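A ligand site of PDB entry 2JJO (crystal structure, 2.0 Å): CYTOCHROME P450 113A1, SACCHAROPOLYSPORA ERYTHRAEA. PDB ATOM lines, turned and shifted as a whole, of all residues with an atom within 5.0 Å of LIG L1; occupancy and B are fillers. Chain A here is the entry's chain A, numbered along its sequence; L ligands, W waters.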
ATOM      1  N   PRO A  73      22.045  -3.184  -3.166  1.00  0.00           N
ATOM      2  CA  PRO A  73      23.316  -3.736  -2.652  1.00  0.00           C
ATOM      3  C   PRO A  73      24.482  -3.425  -3.550  1.00  0.00           C
ATOM      4  O   PRO A  73      25.635  -3.543  -3.142  1.00  0.00           O
ATOM      5  CB  PRO A  73      23.076  -5.265  -2.623  1.00  0.00           C
ATOM      6  CG  PRO A  73      21.978  -5.488  -3.659  1.00  0.00           C
ATOM      7  CD  PRO A  73      21.151  -4.230  -3.711  1.00  0.00           C
ATOM      8  N   THR A  83      20.325  -4.288 -10.807  1.00  0.00           N
ATOM      9  CA  THR A  83      19.513  -5.181 -11.636  1.00  0.00           C
ATOM     10  C   THR A  83      18.231  -4.390 -11.905  1.00  0.00           C
ATOM     11  O   THR A  83      17.474  -4.118 -10.980  1.00  0.00           O
ATOM     12  CB  THR A  83      19.211  -6.494 -10.882  1.00  0.00           C
ATOM     13  OG1 THR A  83      20.424  -7.116 -10.459  1.00  0.00           O
ATOM     14  CG2 THR A  83      18.444  -7.464 -11.770  1.00  0.00           C
ATOM     15  N   MET A  86      14.109  -4.319 -10.189  1.00  0.00           N
ATOM     16  CA  MET A  86      14.088  -5.013  -8.893  1.00  0.00           C
ATOM     17  C   MET A  86      13.543  -4.117  -7.798  1.00  0.00           C
ATOM     18  O   MET A  86      14.296  -3.371  -7.147  1.00  0.00           O
ATOM     19  CB  MET A  86      15.463  -5.586  -8.520  1.00  0.00           C
ATOM     20  CG  MET A  86      15.872  -6.788  -9.364  1.00  0.00           C
ATOM     21  SD  MET A  86      14.569  -8.044  -9.481  1.00  0.00           S
ATOM     22  CE  MET A  86      15.549  -9.506  -9.916  1.00  0.00           C
ATOM     23  N   ILE A  87      12.223  -4.175  -7.617  1.00  0.00           N
ATOM     24  CA  ILE A  87      11.526  -3.275  -6.699  1.00  0.00           C
ATOM     25  C   ILE A  87      12.146  -3.215  -5.266  1.00  0.00           C
ATOM     26  O   ILE A  87      12.306  -2.126  -4.681  1.00  0.00           O
ATOM     27  CB  ILE A  87      10.015  -3.628  -6.670  1.00  0.00           C
ATOM     28  CG1 ILE A  87       9.206  -2.588  -5.898  1.00  0.00           C
ATOM     29  CG2 ILE A  87       9.810  -5.052  -6.127  1.00  0.00           C
ATOM     30  CD1 ILE A  87       7.719  -2.921  -5.802  1.00  0.00           C
ATOM     31  N   HIS A  88      12.545  -4.373  -4.750  1.00  0.00           N
ATOM     32  CA  HIS A  88      13.147  -4.477  -3.431  1.00  0.00           C
ATOM     33  C   HIS A  88      14.563  -3.863  -3.348  1.00  0.00           C
ATOM     34  O   HIS A  88      15.141  -3.810  -2.241  1.00  0.00           O
ATOM     35  CB  HIS A  88      13.174  -5.957  -3.008  1.00  0.00           C
ATOM     36  CG  HIS A  88      14.082  -6.795  -3.871  1.00  0.00           C
ATOM     37  ND1 HIS A  88      13.812  -7.060  -5.207  1.00  0.00           N
ATOM     38  CD2 HIS A  88      15.273  -7.388  -3.606  1.00  0.00           C
ATOM     39  CE1 HIS A  88      14.804  -7.770  -5.720  1.00  0.00           C
ATOM     40  NE2 HIS A  88      15.701  -7.972  -4.772  1.00  0.00           N
ATOM     41  N   GLU A  89      15.118  -3.457  -4.494  1.00  0.00           N
ATOM     42  CA  GLU A  89      16.450  -2.822  -4.545  1.00  0.00           C
ATOM     43  C   GLU A  89      16.462  -1.371  -5.054  1.00  0.00           C
ATOM     44  O   GLU A  89      17.531  -0.820  -5.364  1.00  0.00           O
ATOM     45  CB  GLU A  89      17.420  -3.686  -5.348  1.00  0.00           C
ATOM     46  CG  GLU A  89      17.693  -5.047  -4.654  1.00  0.00           C
ATOM     47  CD  GLU A  89      18.604  -5.975  -5.493  1.00  0.00           C
ATOM     48  OE1 GLU A  89      18.941  -5.617  -6.637  1.00  0.00           O
ATOM     49  OE2 GLU A  89      19.043  -7.025  -4.956  1.00  0.00           O
ATOM     50  N   LEU A 169      18.169 -21.130  -5.307  1.00  0.00           N
ATOM     51  CA  LEU A 169      18.510 -19.808  -4.820  1.00  0.00           C
ATOM     52  C   LEU A 169      18.703 -19.845  -3.300  1.00  0.00           C
ATOM     53  O   LEU A 169      19.717 -19.366  -2.797  1.00  0.00           O
ATOM     54  CB  LEU A 169      17.447 -18.793  -5.224  1.00  0.00           C
ATOM     55  CG  LEU A 169      17.592 -17.339  -4.733  1.00  0.00           C
ATOM     56  CD1 LEU A 169      18.801 -16.662  -5.382  1.00  0.00           C
ATOM     57  CD2 LEU A 169      16.321 -16.515  -4.992  1.00  0.00           C
ATOM     58  N   VAL A 170      17.745 -20.431  -2.580  1.00  0.00           N
ATOM     59  CA  VAL A 170      17.777 -20.446  -1.114  1.00  0.00           C
ATOM     60  C   VAL A 170      18.983 -21.197  -0.584  1.00  0.00           C
ATOM     61  O   VAL A 170      19.511 -20.843   0.485  1.00  0.00           O
ATOM     62  CB  VAL A 170      16.443 -20.974  -0.492  1.00  0.00           C
ATOM     63  CG1 VAL A 170      16.625 -21.326   0.970  1.00  0.00           C
ATOM     64  CG2 VAL A 170      15.375 -19.910  -0.639  1.00  0.00           C
ATOM     65  N   ILE A 172      21.975 -21.504  -2.412  1.00  0.00           N
ATOM     66  CA  ILE A 172      23.161 -21.032  -3.113  1.00  0.00           C
ATOM     67  C   ILE A 172      24.374 -20.952  -2.163  1.00  0.00           C
ATOM     68  O   ILE A 172      24.217 -20.550  -0.992  1.00  0.00           O
ATOM     69  CB  ILE A 172      22.858 -19.679  -3.818  1.00  0.00           C
ATOM     70  CG1 ILE A 172      23.793 -19.451  -5.008  1.00  0.00           C
ATOM     71  CG2 ILE A 172      22.817 -18.456  -2.817  1.00  0.00           C
ATOM     72  CD1 ILE A 172      23.334 -18.386  -5.876  1.00  0.00           C
ATOM     73  N   MET A 174      27.185 -19.418  -0.279  1.00  0.00           N
ATOM     74  CA  MET A 174      27.207 -18.029   0.107  1.00  0.00           C
ATOM     75  C   MET A 174      28.042 -17.929   1.377  1.00  0.00           C
ATOM     76  O   MET A 174      27.938 -18.740   2.264  1.00  0.00           O
ATOM     77  CB  MET A 174      25.770 -17.568   0.388  1.00  0.00           C
ATOM     78  CG  MET A 174      25.618 -16.174   1.020  1.00  0.00           C
ATOM     79  SD  MET A 174      23.921 -15.681   1.247  1.00  0.00           S
ATOM     80  CE  MET A 174      23.439 -16.457   2.765  1.00  0.00           C
ATOM     81  N   PRO A 177      28.410 -11.679   1.709  1.00  0.00           N
ATOM     82  CA  PRO A 177      27.298 -11.191   0.857  1.00  0.00           C
ATOM     83  C   PRO A 177      27.660 -10.005  -0.037  1.00  0.00           C
ATOM     84  O   PRO A 177      26.852  -9.605  -0.909  1.00  0.00           O
ATOM     85  CB  PRO A 177      26.225 -10.818   1.891  1.00  0.00           C
ATOM     86  CG  PRO A 177      27.015 -10.364   3.067  1.00  0.00           C
ATOM     87  CD  PRO A 177      28.230 -11.268   3.126  1.00  0.00           C
ATOM     88  N   LEU A 182      29.327 -13.926  -5.587  1.00  0.00           N
ATOM     89  CA  LEU A 182      27.975 -14.342  -5.150  1.00  0.00           C
ATOM     90  C   LEU A 182      26.907 -13.766  -6.061  1.00  0.00           C
ATOM     91  O   LEU A 182      25.978 -14.449  -6.415  1.00  0.00           O
ATOM     92  CB  LEU A 182      27.708 -13.987  -3.711  1.00  0.00           C
ATOM     93  CG  LEU A 182      26.262 -14.149  -3.217  1.00  0.00           C
ATOM     94  CD1 LEU A 182      25.807 -15.639  -3.160  1.00  0.00           C
ATOM     95  CD2 LEU A 182      26.157 -13.481  -1.840  1.00  0.00           C
ATOM     96  N   ILE A 186      24.178 -15.767  -8.152  1.00  0.00           N
ATOM     97  CA  ILE A 186      22.725 -15.484  -8.085  1.00  0.00           C
ATOM     98  C   ILE A 186      22.123 -15.239  -9.453  1.00  0.00           C
ATOM     99  O   ILE A 186      21.047 -15.761  -9.766  1.00  0.00           O
ATOM    100  CB  ILE A 186      22.394 -14.282  -7.173  1.00  0.00           C
ATOM    101  CG1 ILE A 186      22.806 -14.596  -5.727  1.00  0.00           C
ATOM    102  CG2 ILE A 186      20.899 -13.865  -7.333  1.00  0.00           C
ATOM    103  CD1 ILE A 186      22.738 -13.419  -4.738  1.00  0.00           C
ATOM    104  N   LEU A 190      19.205 -17.656 -11.304  1.00  0.00           N
ATOM    105  CA  LEU A 190      17.894 -17.102 -11.667  1.00  0.00           C
ATOM    106  C   LEU A 190      17.693 -17.014 -13.159  1.00  0.00           C
ATOM    107  O   LEU A 190      16.594 -16.771 -13.627  1.00  0.00           O
ATOM    108  CB  LEU A 190      17.702 -15.713 -11.075  1.00  0.00           C
ATOM    109  CG  LEU A 190      17.546 -15.567  -9.554  1.00  0.00           C
ATOM    110  CD1 LEU A 190      17.365 -14.111  -9.257  1.00  0.00           C
ATOM    111  CD2 LEU A 190      16.352 -16.411  -9.043  1.00  0.00           C
ATOM    112  N   ALA A 237      11.061 -11.208  -9.239  1.00  0.00           N
ATOM    113  CA  ALA A 237      10.924 -10.784  -7.831  1.00  0.00           C
ATOM    114  C   ALA A 237       9.519 -11.086  -7.311  1.00  0.00           C
ATOM    115  O   ALA A 237       9.375 -11.567  -6.200  1.00  0.00           O
ATOM    116  CB  ALA A 237      11.276  -9.259  -7.671  1.00  0.00           C
ATOM    117  N   LEU A 240       9.136 -14.995  -6.679  1.00  0.00           N
ATOM    118  CA  LEU A 240       9.905 -15.437  -5.533  1.00  0.00           C
ATOM    119  C   LEU A 240       9.316 -14.924  -4.219  1.00  0.00           C
ATOM    120  O   LEU A 240       9.221 -15.666  -3.248  1.00  0.00           O
ATOM    121  CB  LEU A 240      11.373 -14.999  -5.699  1.00  0.00           C
ATOM    122  CG  LEU A 240      12.206 -15.695  -6.775  1.00  0.00           C
ATOM    123  CD1 LEU A 240      13.491 -14.916  -6.987  1.00  0.00           C
ATOM    124  CD2 LEU A 240      12.526 -17.236  -6.436  1.00  0.00           C
ATOM    125  N   ALA A 241       8.866 -13.666  -4.217  1.00  0.00           N
ATOM    126  CA  ALA A 241       8.309 -13.037  -3.026  1.00  0.00           C
ATOM    127  C   ALA A 241       6.999 -13.720  -2.656  1.00  0.00           C
ATOM    128  O   ALA A 241       6.619 -13.766  -1.493  1.00  0.00           O
ATOM    129  CB  ALA A 241       8.042 -11.564  -3.285  1.00  0.00           C
ATOM    130  N   ILE A 244       7.902 -18.284  -1.280  1.00  0.00           N
ATOM    131  CA  ILE A 244       8.883 -18.963  -0.437  1.00  0.00           C
ATOM    132  C   ILE A 244       8.562 -18.714   1.056  1.00  0.00           C
ATOM    133  O   ILE A 244       8.473 -19.652   1.839  1.00  0.00           O
ATOM    134  CB  ILE A 244      10.369 -18.549  -0.749  1.00  0.00           C
ATOM    135  CG1 ILE A 244      10.716 -18.848  -2.228  1.00  0.00           C
ATOM    136  CG2 ILE A 244      11.270 -19.275   0.254  1.00  0.00           C
ATOM    137  CD1 ILE A 244      12.059 -18.116  -2.796  1.00  0.00           C
ATOM    138  N   THR A 245       8.380 -17.456   1.438  1.00  0.00           N
ATOM    139  CA  THR A 245       8.139 -17.097   2.854  1.00  0.00           C
ATOM    140  C   THR A 245       6.745 -17.526   3.375  1.00  0.00           C
ATOM    141  O   THR A 245       6.590 -17.816   4.568  1.00  0.00           O
ATOM    142  CB  THR A 245       8.255 -15.580   3.083  1.00  0.00           C
ATOM    143  OG1 THR A 245       7.572 -14.888   2.010  1.00  0.00           O
ATOM    144  CG2 THR A 245       9.689 -15.150   3.075  1.00  0.00           C
ATOM    145  N   PHE A 288      11.943 -14.530   7.102  1.00  0.00           N
ATOM    146  CA  PHE A 288      13.102 -13.834   6.578  1.00  0.00           C
ATOM    147  C   PHE A 288      13.653 -13.051   7.793  1.00  0.00           C
ATOM    148  O   PHE A 288      13.137 -11.978   8.131  1.00  0.00           O
ATOM    149  CB  PHE A 288      12.619 -12.851   5.476  1.00  0.00           C
ATOM    150  CG  PHE A 288      13.698 -12.276   4.627  1.00  0.00           C
ATOM    151  CD1 PHE A 288      14.699 -13.088   4.080  1.00  0.00           C
ATOM    152  CD2 PHE A 288      13.702 -10.910   4.323  1.00  0.00           C
ATOM    153  CE1 PHE A 288      15.714 -12.553   3.265  1.00  0.00           C
ATOM    154  CE2 PHE A 288      14.681 -10.360   3.494  1.00  0.00           C
ATOM    155  CZ  PHE A 288      15.682 -11.188   2.953  1.00  0.00           C
ATOM    156  N   GLN A 290      16.571 -11.581   8.513  1.00  0.00           N
ATOM    157  CA  GLN A 290      17.520 -10.490   8.383  1.00  0.00           C
ATOM    158  C   GLN A 290      17.340  -9.864   6.997  1.00  0.00           C
ATOM    159  O   GLN A 290      16.825 -10.530   6.090  1.00  0.00           O
ATOM    160  CB  GLN A 290      18.945 -11.024   8.586  1.00  0.00           C
ATOM    161  CG  GLN A 290      19.319 -11.980   7.485  1.00  0.00           C
ATOM    162  CD  GLN A 290      20.658 -12.661   7.669  1.00  0.00           C
ATOM    163  OE1 GLN A 290      21.486 -12.264   8.508  1.00  0.00           O
ATOM    164  NE2 GLN A 290      20.884 -13.684   6.843  1.00  0.00           N
ATOM    165  N   GLN A 292      19.198  -6.722   4.112  1.00  0.00           N
ATOM    166  CA  GLN A 292      20.397  -5.907   3.939  1.00  0.00           C
ATOM    167  C   GLN A 292      20.056  -4.540   3.399  1.00  0.00           C
ATOM    168  O   GLN A 292      19.046  -4.398   2.714  1.00  0.00           O
ATOM    169  CB  GLN A 292      21.462  -6.606   3.096  1.00  0.00           C
ATOM    170  CG  GLN A 292      22.104  -7.797   3.773  1.00  0.00           C
ATOM    171  CD  GLN A 292      21.270  -9.058   3.566  1.00  0.00           C
ATOM    172  OE1 GLN A 292      21.064  -9.477   2.418  1.00  0.00           O
ATOM    173  NE2 GLN A 292      20.786  -9.660   4.665  1.00  0.00           N
ATOM    174  N   ILE A 392      19.522 -18.063   5.068  1.00  0.00           N
ATOM    175  CA  ILE A 392      18.616 -17.142   4.401  1.00  0.00           C
ATOM    176  C   ILE A 392      17.210 -17.091   5.033  1.00  0.00           C
ATOM    177  O   ILE A 392      16.723 -16.004   5.363  1.00  0.00           O
ATOM    178  CB  ILE A 392      18.547 -17.371   2.850  1.00  0.00           C
ATOM    179  CG1 ILE A 392      19.948 -17.158   2.229  1.00  0.00           C
ATOM    180  CG2 ILE A 392      17.573 -16.414   2.189  1.00  0.00           C
ATOM    181  CD1 ILE A 392      20.021 -17.427   0.707  1.00  0.00           C
ATOM    182  N   VAL A 393      16.556 -18.248   5.170  1.00  0.00           N
ATOM    183  CA  VAL A 393      15.227 -18.248   5.822  1.00  0.00           C
ATOM    184  C   VAL A 393      15.282 -18.998   7.148  1.00  0.00           C
ATOM    185  O   VAL A 393      16.174 -19.809   7.388  1.00  0.00           O
ATOM    186  CB  VAL A 393      14.126 -18.860   4.937  1.00  0.00           C
ATOM    187  CG1 VAL A 393      13.875 -17.998   3.704  1.00  0.00           C
ATOM    188  CG2 VAL A 393      14.453 -20.335   4.549  1.00  0.00           C
HETATM  189  O1  LIG L   1      12.517 -12.353  -3.384  1.00  0.00           O
HETATM  190  C1  LIG L   1      13.098 -11.256  -3.419  1.00  0.00           C
HETATM  191  O2  LIG L   1      12.574 -10.138  -2.718  1.00  0.00           O
HETATM  192  C2  LIG L   1      11.305 -10.264  -2.069  1.00  0.00           C
HETATM  193  C3  LIG L   1      10.509  -8.986  -2.316  1.00  0.00           C
HETATM  194  C4  LIG L   1      10.455  -8.634  -3.778  1.00  0.00           C
HETATM  195  C5  LIG L   1      11.576 -10.503  -0.598  1.00  0.00           C
HETATM  196  C6  LIG L   1      12.728  -9.643  -0.101  1.00  0.00           C
HETATM  197  C7  LIG L   1      11.838 -11.991  -0.312  1.00  0.00           C
HETATM  198  O3  LIG L   1      10.702 -12.836  -0.595  1.00  0.00           O
HETATM  199  C8  LIG L   1      12.273 -12.270   1.133  1.00  0.00           C
HETATM  200  C9  LIG L   1      11.139 -11.908   2.126  1.00  0.00           C
HETATM  201  C10 LIG L   1      14.368 -10.894  -4.183  1.00  0.00           C
HETATM  202  C11 LIG L   1      14.060 -10.995  -5.673  1.00  0.00           C
HETATM  203  C12 LIG L   1      15.583 -11.705  -3.725  1.00  0.00           C
HETATM  204  O4  LIG L   1      16.747 -11.077  -4.344  1.00  0.00           O
HETATM  205  C13 LIG L   1      17.757 -11.905  -4.865  1.00  0.00           C
HETATM  206  O5  LIG L   1      18.937 -11.663  -4.092  1.00  0.00           O
HETATM  207  C14 LIG L   1      19.513 -10.365  -4.200  1.00  0.00           C
HETATM  208  C15 LIG L   1      20.753 -10.326  -3.297  1.00  0.00           C
HETATM  209  C16 LIG L   1      19.905 -10.158  -5.649  1.00  0.00           C
HETATM  210  O6  LIG L   1      20.504  -8.860  -5.811  1.00  0.00           O
HETATM  211  C17 LIG L   1      18.736 -10.334  -6.643  1.00  0.00           C
HETATM  212  C18 LIG L   1      19.301 -10.317  -8.071  1.00  0.00           C
HETATM  213  O7  LIG L   1      17.854  -9.213  -6.565  1.00  0.00           O
HETATM  214  C19 LIG L   1      17.965 -11.633  -6.363  1.00  0.00           C
HETATM  215  C20 LIG L   1      15.717 -11.786  -2.184  1.00  0.00           C
HETATM  216  C21 LIG L   1      16.338 -10.502  -1.584  1.00  0.00           C
HETATM  217  C22 LIG L   1      16.431 -13.080  -1.756  1.00  0.00           C
HETATM  218  C23 LIG L   1      15.486 -14.260  -1.456  1.00  0.00           C
HETATM  219  C24 LIG L   1      16.270 -15.573  -1.429  1.00  0.00           C
HETATM  220  O8  LIG L   1      14.531 -14.410  -2.543  1.00  0.00           O
HETATM  221  C25 LIG L   1      14.841 -13.984  -0.076  1.00  0.00           C
HETATM  222  C26 LIG L   1      13.427 -14.494   0.179  1.00  0.00           C
HETATM  223  C27 LIG L   1      13.450 -15.998   0.511  1.00  0.00           C
HETATM  224  C28 LIG L   1      12.729 -13.727   1.266  1.00  0.00           C
HETATM  225  O9  LIG L   1      12.468 -14.303   2.293  1.00  0.00           O
HETATM  226  O10 LIG L   1      17.218 -12.913  -0.587  1.00  0.00           O
HETATM  227  C29 LIG L   1      18.624 -12.871  -0.821  1.00  0.00           C
HETATM  228  O11 LIG L   1      19.121 -14.107  -1.347  1.00  0.00           O
HETATM  229  C30 LIG L   1      20.524 -14.053  -1.619  1.00  0.00           C
HETATM  230  C31 LIG L   1      20.916 -15.340  -2.279  1.00  0.00           C
HETATM  231  C32 LIG L   1      21.324 -13.783  -0.334  1.00  0.00           C
HETATM  232  C33 LIG L   1      20.778 -12.528   0.390  1.00  0.00           C
HETATM  233  N1  LIG L   1      21.409 -12.192   1.699  1.00  0.00           N
HETATM  234  C34 LIG L   1      22.829 -11.849   1.496  1.00  0.00           C
HETATM  235  C35 LIG L   1      21.288 -13.202   2.777  1.00  0.00           C
HETATM  236  C36 LIG L   1      19.265 -12.645   0.546  1.00  0.00           C
HETATM  237  O12 LIG L   1      18.751 -11.432   1.129  1.00  0.00           O
HETATM  238  C1  LG2 L   2       8.642  -7.380   0.549  1.00  0.00           C
HETATM  239  C2  LG2 L   2       8.222 -10.716   4.028  1.00  0.00           C
HETATM  240  C3  LG2 L   2       4.639 -12.811   1.501  1.00  0.00           C
HETATM  241  C4  LG2 L   2       5.297  -9.677  -2.134  1.00  0.00           C
HETATM  242  C5  LG2 L   2       8.791  -8.083   1.714  1.00  0.00           C
HETATM  243  C6  LG2 L   2       9.654  -7.668   2.798  1.00  0.00           C
HETATM  244  C7  LG2 L   2       9.551  -8.577   3.759  1.00  0.00           C
HETATM  245  C8  LG2 L   2       8.604  -9.595   3.311  1.00  0.00           C
HETATM  246  C9  LG2 L   2      10.286  -8.602   5.134  1.00  0.00           C
HETATM  247  C10 LG2 L   2      10.520  -6.372   2.804  1.00  0.00           C
HETATM  248  C11 LG2 L   2      11.968  -6.602   2.301  1.00  0.00           C
HETATM  249  C12 LG2 L   2      12.869  -5.396   2.517  1.00  0.00           C
HETATM  250  O1  LG2 L   2      12.466  -4.445   3.281  1.00  0.00           O
HETATM  251  O2  LG2 L   2      14.039  -5.392   1.963  1.00  0.00           O
HETATM  252  C13 LG2 L   2       7.189 -11.573   3.648  1.00  0.00           C
HETATM  253  C14 LG2 L   2       6.709 -12.667   4.434  1.00  0.00           C
HETATM  254  C15 LG2 L   2       5.717 -13.265   3.754  1.00  0.00           C
HETATM  255  C16 LG2 L   2       5.525 -12.522   2.501  1.00  0.00           C
HETATM  256  C17 LG2 L   2       7.294 -13.061   5.830  1.00  0.00           C
HETATM  257  C18 LG2 L   2       4.909 -14.521   4.199  1.00  0.00           C
HETATM  258  C19 LG2 L   2       4.607 -14.747   5.508  1.00  0.00           C
HETATM  259  C20 LG2 L   2       4.516 -12.162   0.285  1.00  0.00           C
HETATM  260  C21 LG2 L   2       3.594 -12.538  -0.781  1.00  0.00           C
HETATM  261  C22 LG2 L   2       3.756 -11.648  -1.775  1.00  0.00           C
HETATM  262  C23 LG2 L   2       4.823 -10.720  -1.397  1.00  0.00           C
HETATM  263  C24 LG2 L   2       2.571 -13.707  -0.682  1.00  0.00           C
HETATM  264  C25 LG2 L   2       3.016 -11.622  -3.128  1.00  0.00           C
HETATM  265  C26 LG2 L   2       3.728 -11.578  -4.265  1.00  0.00           C
HETATM  266  C27 LG2 L   2       6.260  -8.778  -1.768  1.00  0.00           C
HETATM  267  C28 LG2 L   2       6.787  -7.731  -2.614  1.00  0.00           C
HETATM  268  C29 LG2 L   2       7.801  -7.020  -1.753  1.00  0.00           C
HETATM  269  C30 LG2 L   2       7.823  -7.726  -0.506  1.00  0.00           C
HETATM  270  C31 LG2 L   2       6.370  -7.374  -4.077  1.00  0.00           C
HETATM  271  C32 LG2 L   2       8.704  -5.835  -2.122  1.00  0.00           C
HETATM  272  C33 LG2 L   2       7.971  -4.593  -1.671  1.00  0.00           C
HETATM  273  C34 LG2 L   2       8.767  -3.362  -2.006  1.00  0.00           C
HETATM  274  O3  LG2 L   2      10.031  -3.439  -2.067  1.00  0.00           O
HETATM  275  O4  LG2 L   2       8.167  -2.278  -2.204  1.00  0.00           O
HETATM  276  N1  LG2 L   2       8.158  -9.243   2.048  1.00  0.00           N
HETATM  277  N2  LG2 L   2       6.467 -11.522   2.449  1.00  0.00           N
HETATM  278  N3  LG2 L   2       5.263 -11.064  -0.131  1.00  0.00           N
HETATM  279  N4  LG2 L   2       6.905  -8.752  -0.548  1.00  0.00           N
HETATM  280 FE1  LG2 L   2       6.574 -10.015   1.045  1.00  0.00          FE
HETATM  281  O   HOH W   1       9.468 -15.239  -0.639  1.00  0.00           O
HETATM  282  O   HOH W   2      21.061 -10.002 -11.045  1.00  0.00           O
HETATM  283  O   HOH W   3       8.063 -12.048   0.410  1.00  0.00           O
HETATM  284  O   HOH W   4      23.205  -9.173  -6.133  1.00  0.00           O
HETATM  285  O   HOH W   5      18.562 -11.338   3.993  1.00  0.00           O
HETATM  286  O   HOH W   6      21.123  -6.561  -7.929  1.00  0.00           O
HETATM  287  O   HOH W   7      19.266  -9.033  -0.161  1.00  0.00           O
HETATM  288  O   HOH W   8      18.602 -13.992   4.863  1.00  0.00           O
HETATM  289  O   HOH W   9      23.752 -12.200   4.636  1.00  0.00           O
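Water W1 lies within hydrogen-bond range of the backbone carbonyl oxygen (O) of Leu 240 (2.7 Å), an oxygen (O3) of LIG L1 (2.7 Å), the backbone NH (N) of Thr 245 (3.2 Å), the backbone carbonyl oxygen (O) of Ala 241 (3.3 Å) and the backbone NH (N) of Ile 244 (3.5 Å).
Water W7 bridges O12 of LIG L1 and OE1 of Gln 292.
Water W5 lies within hydrogen-bond range of the backbone carbonyl oxygen of Gln 290 (2.8 Å), the side-chain amide nitrogen of Gln 292 (2.9 Å) and an oxygen (O12) of LIG L1 (2.9 Å).
Water W3 lies within hydrogen-bond range of O3 of LIG L1, O of Ala 241 and OG1 of Thr 245.
Water W6 lies within hydrogen-bond range of OG1 of Thr 83, OE1 of Glu 89 and O6 of LIG L1.
Water W8 bridges the backbone carbonyl oxygen of Ile 392 (2.8 Å) and the side-chain amide nitrogen of Gln 290 (3.0 Å).
A ring nitrogen (NE2) of His 88 lies within hydrogen-bond range of the side-chain carboxylate (OE2) of Glu 89, at 3.5 Å.
Merely in contact with LIG L1: Leu 169 (3.7 Å), Ile 172 (3.7 Å), Met 174 (3.6 Å), Pro 177 (3.6 Å), Ile 186 (3.6 Å), Leu 190 (3.9 Å), Ala 237 (3.8 Å), Leu 240 (3.7 Å), Ala 241 (3.4 Å), Ile 244 (3.9 Å), Thr 245 (3.0 Å), Phe 288 (3.1 Å), Ile 392 (3.8 Å) and Val 393 (3.8 Å).
17 residues have an atom within 4 Å of LIG L1: His 88, Glu 89, Leu 169, Ile 172, Met 174, Pro 177, Ile 186, Leu 190, Ala 237, Leu 240, Ala 241, Ile 244, Thr 245, Phe 288, Gln 292, Ile 392 and Val 393.
The nearest printed residue that does not touch LIG L1 is Met 86 (4.1 Å).
An oxygen (O6) of LIG L1 sits at hydrogen-bond distance from the side-chain carboxylate of Glu 89, at 2.5 Å.
The side-chain amide oxygen of Gln 292 sits close to an oxygen (O12) of LIG L1 (3.3 Å).
NE2 of His 88 is in hydrogen-bond range of O7 of LIG L1, at 3.1 Å.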
